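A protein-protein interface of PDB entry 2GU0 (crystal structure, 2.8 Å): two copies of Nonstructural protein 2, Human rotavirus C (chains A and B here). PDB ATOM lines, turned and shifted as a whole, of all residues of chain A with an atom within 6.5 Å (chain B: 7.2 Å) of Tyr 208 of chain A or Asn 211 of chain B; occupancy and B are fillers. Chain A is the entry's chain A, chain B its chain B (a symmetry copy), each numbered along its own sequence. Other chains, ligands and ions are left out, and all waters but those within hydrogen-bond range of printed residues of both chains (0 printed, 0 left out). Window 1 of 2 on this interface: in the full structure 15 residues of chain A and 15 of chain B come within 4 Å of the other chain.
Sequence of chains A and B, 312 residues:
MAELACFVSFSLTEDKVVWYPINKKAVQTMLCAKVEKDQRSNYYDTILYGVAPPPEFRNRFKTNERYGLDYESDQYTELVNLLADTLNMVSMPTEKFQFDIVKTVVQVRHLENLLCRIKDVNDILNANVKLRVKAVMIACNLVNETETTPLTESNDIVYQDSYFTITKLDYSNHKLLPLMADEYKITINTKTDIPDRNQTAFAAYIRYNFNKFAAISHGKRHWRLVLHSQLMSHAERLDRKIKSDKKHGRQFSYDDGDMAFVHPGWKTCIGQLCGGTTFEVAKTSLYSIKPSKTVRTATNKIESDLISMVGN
The side-chain amide nitrogen of Asn 211 of chain A sits at hydrogen-bond distance from the backbone carbonyl oxygen of Tyr 208 of chain B, at 3.1 Å.
OD1 of Asn 211 of chain A sits close to OD1 of Asn 211 of chain B, at 2.5 Å.
OD1 of Asn 209 of chain A sits at hydrogen-bond distance from NZ of Lys 212 of chain B (3.4 Å).
The side-chain amino group of Lys 212 of chain A is in hydrogen-bond range of the side-chain amide oxygen of Asn 209 of chain B.
ND2 of Asn 211 of chain B sits at hydrogen-bond distance from O of Tyr 208 of chain A, 3.0 Å away.
Tyr 208 of chain A touches Asn 211 of chain B, and with the chains exchanged Asn 211 of chain A touches Tyr 208 of chain B.
Tyr 208 of chain A touches Lys 212 of chain B, and with the chains exchanged Lys 212 of chain A touches Tyr 208 of chain B.
Asn 209 of chain A touches Lys 212 of chain B, and with the chains exchanged Lys 212 of chain A touches Asn 209 of chain B.
Asn 211 of chain A touches its own counterpart, Asn 211 of chain B.
Positions printed for both chains: 205, 206, 207, 208, 209, 210, 211 and 212.
Of the 11 pairs that touch across the chains among the printed residues, 7 have their exchanged pair printed and touching as well.
Tyr 208 of chain A touches just these residues of chain B: Asn 211, Lys 212 and His 228.
Printed residues of chain B within 4 Å of Lys 212 of chain A: Tyr 208 and Asn 209.
Of the printed residues of chain B, Glu 303 of chain A touches His 228 (3.2 Å).
Of the printed residues of chain B, Leu 306 of chain A touches His 228 and Ser 229.
Of the printed residues of chain A, Tyr 208 of chain B touches Asn 211 and Lys 212.
Of the printed residues of chain A, Asn 209 of chain B touches Lys 212 (3.0 Å).
Asn 211 of chain B touches just these residues of chain A: Tyr 208 (3.0 Å) and Asn 211 (2.5 Å).
The nearest printed residue of chain A that does not touch His 228 of chain B is Ile 302 of chain A (6.5 Å).
Among the printed residues, 11 pairs touch across the chains.
Among the printed residues, no Asp or Glu carboxylate lies within 4 Å of a Lys or Arg side-chain nitrogen of the other chain.
ND2 of Asn 209 of chain A sits at hydrogen-bond distance from O of Tyr 205 of chain A (3.0 Å).
The side-chain amide nitrogen of Asn 209 of chain B lies close to the backbone carbonyl oxygen of Tyr 205 of chain B.
The backbone carbonyl oxygen of Lys 212 of chain B is in hydrogen-bond range of the backbone NH of His 228 of chain B (2.9 Å).
A ring nitrogen (NE2) of His 228 of chain B is in hydrogen-bond range of the backbone carbonyl oxygen (O) of Asn 211 of chain B.
Tyr 208 of chain A touches Lys 212 of chain B.
Tyr 208 of chain A touches His 228 of chain B.
Tyr 208 of chain B touches Lys 212 of chain A (OH to CA, 3.4 Å).
Glu 303 of chain A touches His 228 of chain B (OE2 to CE1, 3.2 Å).
Leu 306 of chain A touches His 228 of chain B (O to O, 3.7 Å).
Leu 306 of chain A touches Ser 229 of chain B.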
ATOM      1  N   ALA A 203     -16.965 -15.029  41.157  1.00  0.00           N
ATOM      2  CA  ALA A 203     -15.515 -14.859  41.251  1.00  0.00           C
ATOM      3  C   ALA A 203     -14.853 -15.435  40.011  1.00  0.00           C
ATOM      4  O   ALA A 203     -13.945 -14.834  39.435  1.00  0.00           O
ATOM      5  CB  ALA A 203     -14.991 -15.570  42.495  1.00  0.00           C
ATOM      6  N   ALA A 204     -15.322 -16.613  39.614  1.00  0.00           N
ATOM      7  CA  ALA A 204     -14.813 -17.290  38.437  1.00  0.00           C
ATOM      8  C   ALA A 204     -15.298 -16.537  37.212  1.00  0.00           C
ATOM      9  O   ALA A 204     -14.568 -16.389  36.240  1.00  0.00           O
ATOM     10  CB  ALA A 204     -15.317 -18.718  38.402  1.00  0.00           C
ATOM     11  N   TYR A 205     -16.534 -16.048  37.264  1.00  0.00           N
ATOM     12  CA  TYR A 205     -17.078 -15.309  36.138  1.00  0.00           C
ATOM     13  C   TYR A 205     -16.219 -14.109  35.781  1.00  0.00           C
ATOM     14  O   TYR A 205     -15.902 -13.913  34.613  1.00  0.00           O
ATOM     15  CB  TYR A 205     -18.499 -14.812  36.405  1.00  0.00           C
ATOM     16  CG  TYR A 205     -19.050 -14.031  35.233  1.00  0.00           C
ATOM     17  CD1 TYR A 205     -19.666 -14.678  34.172  1.00  0.00           C
ATOM     18  CD2 TYR A 205     -18.855 -12.649  35.135  1.00  0.00           C
ATOM     19  CE1 TYR A 205     -20.070 -13.970  33.030  1.00  0.00           C
ATOM     20  CE2 TYR A 205     -19.250 -11.932  33.999  1.00  0.00           C
ATOM     21  CZ  TYR A 205     -19.852 -12.600  32.955  1.00  0.00           C
ATOM     22  OH  TYR A 205     -20.216 -11.912  31.829  1.00  0.00           O
ATOM     23  N   ILE A 206     -15.844 -13.298  36.763  1.00  0.00           N
ATOM     24  CA  ILE A 206     -15.041 -12.125  36.436  1.00  0.00           C
ATOM     25  C   ILE A 206     -13.579 -12.437  36.147  1.00  0.00           C
ATOM     26  O   ILE A 206     -12.874 -11.621  35.553  1.00  0.00           O
ATOM     27  CB  ILE A 206     -15.110 -11.023  37.532  1.00  0.00           C
ATOM     28  CG1 ILE A 206     -14.671 -11.583  38.882  1.00  0.00           C
ATOM     29  CG2 ILE A 206     -16.519 -10.439  37.602  1.00  0.00           C
ATOM     30  CD1 ILE A 206     -14.655 -10.541  39.977  1.00  0.00           C
ATOM     31  N   ARG A 207     -13.111 -13.610  36.557  1.00  0.00           N
ATOM     32  CA  ARG A 207     -11.723 -13.945  36.277  1.00  0.00           C
ATOM     33  C   ARG A 207     -11.571 -14.149  34.787  1.00  0.00           C
ATOM     34  O   ARG A 207     -10.603 -13.690  34.188  1.00  0.00           O
ATOM     35  CB  ARG A 207     -11.292 -15.208  37.002  1.00  0.00           C
ATOM     36  CG  ARG A 207     -10.714 -14.977  38.376  1.00  0.00           C
ATOM     37  CD  ARG A 207      -9.589 -15.969  38.650  1.00  0.00           C
ATOM     38  NE  ARG A 207      -8.275 -15.375  38.418  1.00  0.00           N
ATOM     39  CZ  ARG A 207      -7.169 -16.064  38.161  1.00  0.00           C
ATOM     40  NH1 ARG A 207      -7.203 -17.389  38.090  1.00  0.00           N
ATOM     41  NH2 ARG A 207      -6.021 -15.419  37.983  1.00  0.00           N
ATOM     42  N   TYR A 208     -12.545 -14.823  34.188  1.00  0.00           N
ATOM     43  CA  TYR A 208     -12.509 -15.083  32.758  1.00  0.00           C
ATOM     44  C   TYR A 208     -12.985 -13.895  31.896  1.00  0.00           C
ATOM     45  O   TYR A 208     -12.426 -13.639  30.828  1.00  0.00           O
ATOM     46  CB  TYR A 208     -13.330 -16.339  32.444  1.00  0.00           C
ATOM     47  CG  TYR A 208     -13.368 -16.687  30.981  1.00  0.00           C
ATOM     48  CD1 TYR A 208     -12.270 -17.270  30.350  1.00  0.00           C
ATOM     49  CD2 TYR A 208     -14.487 -16.392  30.211  1.00  0.00           C
ATOM     50  CE1 TYR A 208     -12.288 -17.546  28.982  1.00  0.00           C
ATOM     51  CE2 TYR A 208     -14.517 -16.663  28.851  1.00  0.00           C
ATOM     52  CZ  TYR A 208     -13.417 -17.236  28.238  1.00  0.00           C
ATOM     53  OH  TYR A 208     -13.454 -17.482  26.884  1.00  0.00           O
ATOM     54  N   ASN A 209     -13.991 -13.158  32.367  1.00  0.00           N
ATOM     55  CA  ASN A 209     -14.531 -12.012  31.615  1.00  0.00           C
ATOM     56  C   ASN A 209     -13.844 -10.658  31.828  1.00  0.00           C
ATOM     57  O   ASN A 209     -14.022  -9.743  31.026  1.00  0.00           O
ATOM     58  CB  ASN A 209     -16.020 -11.860  31.906  1.00  0.00           C
ATOM     59  CG  ASN A 209     -16.842 -12.915  31.224  1.00  0.00           C
ATOM     60  OD1 ASN A 209     -17.127 -12.809  30.026  1.00  0.00           O
ATOM     61  ND2 ASN A 209     -17.212 -13.961  31.969  1.00  0.00           N
ATOM     62  N   PHE A 210     -13.087 -10.527  32.913  1.00  0.00           N
ATOM     63  CA  PHE A 210     -12.376  -9.293  33.228  1.00  0.00           C
ATOM     64  C   PHE A 210     -11.031  -9.690  33.815  1.00  0.00           C
ATOM     65  O   PHE A 210     -10.697  -9.285  34.926  1.00  0.00           O
ATOM     66  CB  PHE A 210     -13.137  -8.473  34.274  1.00  0.00           C
ATOM     67  CG  PHE A 210     -14.533  -8.097  33.868  1.00  0.00           C
ATOM     68  CD1 PHE A 210     -15.555  -9.043  33.872  1.00  0.00           C
ATOM     69  CD2 PHE A 210     -14.826  -6.796  33.467  1.00  0.00           C
ATOM     70  CE1 PHE A 210     -16.845  -8.705  33.482  1.00  0.00           C
ATOM     71  CE2 PHE A 210     -16.116  -6.448  33.074  1.00  0.00           C
ATOM     72  CZ  PHE A 210     -17.128  -7.408  33.082  1.00  0.00           C
ATOM     73  N   ASN A 211     -10.259 -10.478  33.072  1.00  0.00           N
ATOM     74  CA  ASN A 211      -8.976 -10.944  33.580  1.00  0.00           C
ATOM     75  C   ASN A 211      -7.969  -9.835  33.834  1.00  0.00           C
ATOM     76  O   ASN A 211      -7.100  -9.978  34.686  1.00  0.00           O
ATOM     77  CB  ASN A 211      -8.375 -12.016  32.651  1.00  0.00           C
ATOM     78  CG  ASN A 211      -7.582 -11.432  31.495  1.00  0.00           C
ATOM     79  OD1 ASN A 211      -8.146 -10.912  30.532  1.00  0.00           O
ATOM     80  ND2 ASN A 211      -6.256 -11.521  31.588  1.00  0.00           N
ATOM     81  N   LYS A 212      -8.086  -8.727  33.110  1.00  0.00           N
ATOM     82  CA  LYS A 212      -7.166  -7.600  33.289  1.00  0.00           C
ATOM     83  C   LYS A 212      -7.488  -6.774  34.541  1.00  0.00           C
ATOM     84  O   LYS A 212      -6.708  -5.902  34.944  1.00  0.00           O
ATOM     85  CB  LYS A 212      -7.213  -6.674  32.068  1.00  0.00           C
ATOM     86  CG  LYS A 212      -6.510  -7.194  30.831  1.00  0.00           C
ATOM     87  CD  LYS A 212      -6.624  -6.174  29.709  1.00  0.00           C
ATOM     88  CE  LYS A 212      -5.742  -6.527  28.510  1.00  0.00           C
ATOM     89  NZ  LYS A 212      -5.918  -5.574  27.353  1.00  0.00           N
ATOM     90  N   THR A 299     -12.481 -21.086  36.917  1.00  0.00           N
ATOM     91  CA  THR A 299     -12.340 -20.264  35.721  1.00  0.00           C
ATOM     92  C   THR A 299     -11.887 -21.073  34.497  1.00  0.00           C
ATOM     93  O   THR A 299     -12.305 -20.785  33.376  1.00  0.00           O
ATOM     94  CB  THR A 299     -11.383 -19.069  35.955  1.00  0.00           C
ATOM     95  OG1 THR A 299     -10.045 -19.538  36.110  1.00  0.00           O
ATOM     96  CG2 THR A 299     -11.775 -18.328  37.200  1.00  0.00           C
ATOM     97  N   ILE A 302     -14.834 -22.597  32.994  1.00  0.00           N
ATOM     98  CA  ILE A 302     -15.651 -21.709  32.183  1.00  0.00           C
ATOM     99  C   ILE A 302     -15.125 -21.755  30.768  1.00  0.00           C
ATOM    100  O   ILE A 302     -15.884 -21.915  29.820  1.00  0.00           O
ATOM    101  CB  ILE A 302     -15.594 -20.246  32.654  1.00  0.00           C
ATOM    102  CG1 ILE A 302     -16.325 -20.097  33.984  1.00  0.00           C
ATOM    103  CG2 ILE A 302     -16.230 -19.328  31.602  1.00  0.00           C
ATOM    104  CD1 ILE A 302     -16.366 -18.680  34.486  1.00  0.00           C
ATOM    105  N   GLU A 303     -13.812 -21.611  30.632  1.00  0.00           N
ATOM    106  CA  GLU A 303     -13.185 -21.644  29.324  1.00  0.00           C
ATOM    107  C   GLU A 303     -13.510 -22.946  28.631  1.00  0.00           C
ATOM    108  O   GLU A 303     -13.920 -22.955  27.474  1.00  0.00           O
ATOM    109  CB  GLU A 303     -11.674 -21.518  29.438  1.00  0.00           C
ATOM    110  CG  GLU A 303     -11.048 -21.276  28.092  1.00  0.00           C
ATOM    111  CD  GLU A 303      -9.549 -21.248  28.140  1.00  0.00           C
ATOM    112  OE1 GLU A 303      -8.997 -20.528  29.000  1.00  0.00           O
ATOM    113  OE2 GLU A 303      -8.921 -21.943  27.306  1.00  0.00           O
ATOM    114  N   LEU A 306     -17.073 -23.452  27.667  1.00  0.00           N
ATOM    115  CA  LEU A 306     -17.340 -22.506  26.606  1.00  0.00           C
ATOM    116  C   LEU A 306     -16.811 -23.056  25.277  1.00  0.00           C
ATOM    117  O   LEU A 306     -17.375 -22.786  24.217  1.00  0.00           O
ATOM    118  CB  LEU A 306     -16.692 -21.167  26.954  1.00  0.00           C
ATOM    119  CG  LEU A 306     -17.278 -19.929  26.273  1.00  0.00           C
ATOM    120  CD1 LEU A 306     -18.784 -19.936  26.422  1.00  0.00           C
ATOM    121  CD2 LEU A 306     -16.678 -18.670  26.887  1.00  0.00           C
ATOM    122  N   TYR B 205       1.846 -12.522  26.242  1.00  0.00           N
ATOM    123  CA  TYR B 205       1.117 -11.296  25.949  1.00  0.00           C
ATOM    124  C   TYR B 205      -0.277 -11.653  25.451  1.00  0.00           C
ATOM    125  O   TYR B 205      -1.273 -11.134  25.936  1.00  0.00           O
ATOM    126  CB  TYR B 205       1.835 -10.495  24.875  1.00  0.00           C
ATOM    127  CG  TYR B 205       1.062  -9.282  24.455  1.00  0.00           C
ATOM    128  CD1 TYR B 205       1.153  -8.092  25.170  1.00  0.00           C
ATOM    129  CD2 TYR B 205       0.172  -9.344  23.386  1.00  0.00           C
ATOM    130  CE1 TYR B 205       0.374  -6.992  24.834  1.00  0.00           C
ATOM    131  CE2 TYR B 205      -0.615  -8.258  23.047  1.00  0.00           C
ATOM    132  CZ  TYR B 205      -0.511  -7.083  23.771  1.00  0.00           C
ATOM    133  OH  TYR B 205      -1.284  -5.999  23.415  1.00  0.00           O
ATOM    134  N   ILE B 206      -0.322 -12.536  24.462  1.00  0.00           N
ATOM    135  CA  ILE B 206      -1.558 -13.015  23.863  1.00  0.00           C
ATOM    136  C   ILE B 206      -2.529 -13.575  24.912  1.00  0.00           C
ATOM    137  O   ILE B 206      -3.727 -13.306  24.879  1.00  0.00           O
ATOM    138  CB  ILE B 206      -1.224 -14.117  22.812  1.00  0.00           C
ATOM    139  CG1 ILE B 206      -0.647 -13.467  21.566  1.00  0.00           C
ATOM    140  CG2 ILE B 206      -2.452 -14.912  22.421  1.00  0.00           C
ATOM    141  CD1 ILE B 206      -1.583 -12.470  20.929  1.00  0.00           C
ATOM    142  N   ARG B 207      -2.003 -14.345  25.854  1.00  0.00           N
ATOM    143  CA  ARG B 207      -2.839 -14.958  26.879  1.00  0.00           C
ATOM    144  C   ARG B 207      -3.406 -13.977  27.885  1.00  0.00           C
ATOM    145  O   ARG B 207      -4.414 -14.255  28.539  1.00  0.00           O
ATOM    146  CB  ARG B 207      -2.049 -16.037  27.614  1.00  0.00           C
ATOM    147  CG  ARG B 207      -2.915 -16.993  28.385  1.00  0.00           C
ATOM    148  CD  ARG B 207      -2.312 -18.374  28.363  1.00  0.00           C
ATOM    149  NE  ARG B 207      -3.218 -19.348  28.958  1.00  0.00           N
ATOM    150  CZ  ARG B 207      -3.537 -19.380  30.245  1.00  0.00           C
ATOM    151  NH1 ARG B 207      -3.015 -18.486  31.077  1.00  0.00           N
ATOM    152  NH2 ARG B 207      -4.376 -20.304  30.696  1.00  0.00           N
ATOM    153  N   TYR B 208      -2.756 -12.828  28.013  1.00  0.00           N
ATOM    154  CA  TYR B 208      -3.213 -11.816  28.947  1.00  0.00           C
ATOM    155  C   TYR B 208      -4.209 -10.866  28.282  1.00  0.00           C
ATOM    156  O   TYR B 208      -5.339 -10.697  28.754  1.00  0.00           O
ATOM    157  CB  TYR B 208      -2.026 -11.020  29.481  1.00  0.00           C
ATOM    158  CG  TYR B 208      -2.419 -10.033  30.544  1.00  0.00           C
ATOM    159  CD1 TYR B 208      -2.824 -10.465  31.807  1.00  0.00           C
ATOM    160  CD2 TYR B 208      -2.443  -8.667  30.274  1.00  0.00           C
ATOM    161  CE1 TYR B 208      -3.251  -9.558  32.781  1.00  0.00           C
ATOM    162  CE2 TYR B 208      -2.868  -7.751  31.234  1.00  0.00           C
ATOM    163  CZ  TYR B 208      -3.274  -8.203  32.485  1.00  0.00           C
ATOM    164  OH  TYR B 208      -3.738  -7.309  33.421  1.00  0.00           O
ATOM    165  N   ASN B 209      -3.787 -10.272  27.172  1.00  0.00           N
ATOM    166  CA  ASN B 209      -4.598  -9.308  26.430  1.00  0.00           C
ATOM    167  C   ASN B 209      -5.703  -9.858  25.539  1.00  0.00           C
ATOM    168  O   ASN B 209      -6.507  -9.086  25.006  1.00  0.00           O
ATOM    169  CB  ASN B 209      -3.681  -8.433  25.582  1.00  0.00           C
ATOM    170  CG  ASN B 209      -2.727  -7.625  26.423  1.00  0.00           C
ATOM    171  OD1 ASN B 209      -3.091  -6.574  26.944  1.00  0.00           O
ATOM    172  ND2 ASN B 209      -1.503  -8.122  26.584  1.00  0.00           N
ATOM    173  N   PHE B 210      -5.738 -11.174  25.354  1.00  0.00           N
ATOM    174  CA  PHE B 210      -6.766 -11.790  24.517  1.00  0.00           C
ATOM    175  C   PHE B 210      -7.166 -13.131  25.113  1.00  0.00           C
ATOM    176  O   PHE B 210      -7.477 -14.063  24.388  1.00  0.00           O
ATOM    177  CB  PHE B 210      -6.253 -12.011  23.084  1.00  0.00           C
ATOM    178  CG  PHE B 210      -5.891 -10.741  22.345  1.00  0.00           C
ATOM    179  CD1 PHE B 210      -4.652 -10.125  22.539  1.00  0.00           C
ATOM    180  CD2 PHE B 210      -6.778 -10.174  21.438  1.00  0.00           C
ATOM    181  CE1 PHE B 210      -4.301  -8.964  21.838  1.00  0.00           C
ATOM    182  CE2 PHE B 210      -6.441  -9.007  20.728  1.00  0.00           C
ATOM    183  CZ  PHE B 210      -5.198  -8.405  20.931  1.00  0.00           C
ATOM    184  N   ASN B 211      -7.179 -13.211  26.439  1.00  0.00           N
ATOM    185  CA  ASN B 211      -7.489 -14.451  27.139  1.00  0.00           C
ATOM    186  C   ASN B 211      -8.744 -15.189  26.727  1.00  0.00           C
ATOM    187  O   ASN B 211      -8.886 -16.359  27.058  1.00  0.00           O
ATOM    188  CB  ASN B 211      -7.553 -14.215  28.648  1.00  0.00           C
ATOM    189  CG  ASN B 211      -8.803 -13.476  29.063  1.00  0.00           C
ATOM    190  OD1 ASN B 211      -9.029 -12.350  28.630  1.00  0.00           O
ATOM    191  ND2 ASN B 211      -9.623 -14.104  29.901  1.00  0.00           N
ATOM    192  N   LYS B 212      -9.668 -14.542  26.027  1.00  0.00           N
ATOM    193  CA  LYS B 212     -10.886 -15.257  25.649  1.00  0.00           C
ATOM    194  C   LYS B 212     -10.771 -15.864  24.280  1.00  0.00           C
ATOM    195  O   LYS B 212     -11.698 -16.522  23.799  1.00  0.00           O
ATOM    196  CB  LYS B 212     -12.109 -14.340  25.715  1.00  0.00           C
ATOM    197  CG  LYS B 212     -12.372 -13.841  27.115  1.00  0.00           C
ATOM    198  CD  LYS B 212     -13.842 -13.585  27.389  1.00  0.00           C
ATOM    199  CE  LYS B 212     -14.379 -12.413  26.613  1.00  0.00           C
ATOM    200  NZ  LYS B 212     -15.805 -12.178  26.988  1.00  0.00           N
ATOM    201  N   PHE B 213      -9.614 -15.653  23.665  1.00  0.00           N
ATOM    202  CA  PHE B 213      -9.329 -16.172  22.334  1.00  0.00           C
ATOM    203  C   PHE B 213      -8.267 -17.262  22.356  1.00  0.00           C
ATOM    204  O   PHE B 213      -7.459 -17.363  23.284  1.00  0.00           O
ATOM    205  CB  PHE B 213      -8.838 -15.058  21.413  1.00  0.00           C
ATOM    206  CG  PHE B 213      -9.710 -13.854  21.403  1.00  0.00           C
ATOM    207  CD1 PHE B 213      -9.746 -13.002  22.490  1.00  0.00           C
ATOM    208  CD2 PHE B 213     -10.515 -13.578  20.312  1.00  0.00           C
ATOM    209  CE1 PHE B 213     -10.568 -11.895  22.491  1.00  0.00           C
ATOM    210  CE2 PHE B 213     -11.347 -12.463  20.306  1.00  0.00           C
ATOM    211  CZ  PHE B 213     -11.371 -11.624  21.399  1.00  0.00           C
ATOM    212  N   ALA B 214      -8.284 -18.076  21.312  1.00  0.00           N
ATOM    213  CA  ALA B 214      -7.324 -19.150  21.132  1.00  0.00           C
ATOM    214  C   ALA B 214      -6.681 -18.840  19.798  1.00  0.00           C
ATOM    215  O   ALA B 214      -7.368 -18.510  18.830  1.00  0.00           O
ATOM    216  CB  ALA B 214      -8.035 -20.496  21.075  1.00  0.00           C
ATOM    217  N   LEU B 227     -12.722 -16.636  19.508  1.00  0.00           N
ATOM    218  CA  LEU B 227     -13.298 -16.850  20.833  1.00  0.00           C
ATOM    219  C   LEU B 227     -13.323 -18.340  21.159  1.00  0.00           C
ATOM    220  O   LEU B 227     -13.589 -19.152  20.284  1.00  0.00           O
ATOM    221  CB  LEU B 227     -14.740 -16.339  20.895  1.00  0.00           C
ATOM    222  CG  LEU B 227     -15.130 -14.898  21.210  1.00  0.00           C
ATOM    223  CD1 LEU B 227     -14.022 -14.240  22.025  1.00  0.00           C
ATOM    224  CD2 LEU B 227     -15.414 -14.148  19.924  1.00  0.00           C
ATOM    225  N   HIS B 228     -13.059 -18.697  22.414  1.00  0.00           N
ATOM    226  CA  HIS B 228     -13.096 -20.103  22.824  1.00  0.00           C
ATOM    227  C   HIS B 228     -14.434 -20.725  22.417  1.00  0.00           C
ATOM    228  O   HIS B 228     -14.519 -21.904  22.042  1.00  0.00           O
ATOM    229  CB  HIS B 228     -12.934 -20.221  24.337  1.00  0.00           C
ATOM    230  CG  HIS B 228     -11.595 -19.781  24.841  1.00  0.00           C
ATOM    231  ND1 HIS B 228     -10.415 -20.358  24.423  1.00  0.00           N
ATOM    232  CD2 HIS B 228     -11.252 -18.824  25.732  1.00  0.00           C
ATOM    233  CE1 HIS B 228      -9.402 -19.774  25.034  1.00  0.00           C
ATOM    234  NE2 HIS B 228      -9.883 -18.840  25.834  1.00  0.00           N
ATOM    235  N   SER B 229     -15.482 -19.918  22.491  1.00  0.00           N
ATOM    236  CA  SER B 229     -16.806 -20.367  22.133  1.00  0.00           C
ATOM    237  C   SER B 229     -16.887 -20.657  20.637  1.00  0.00           C
ATOM    238  O   SER B 229     -17.950 -20.971  20.124  1.00  0.00           O
ATOM    239  CB  SER B 229     -17.816 -19.288  22.483  1.00  0.00           C
ATOM    240  OG  SER B 229     -17.693 -18.204  21.574  1.00  0.00           O
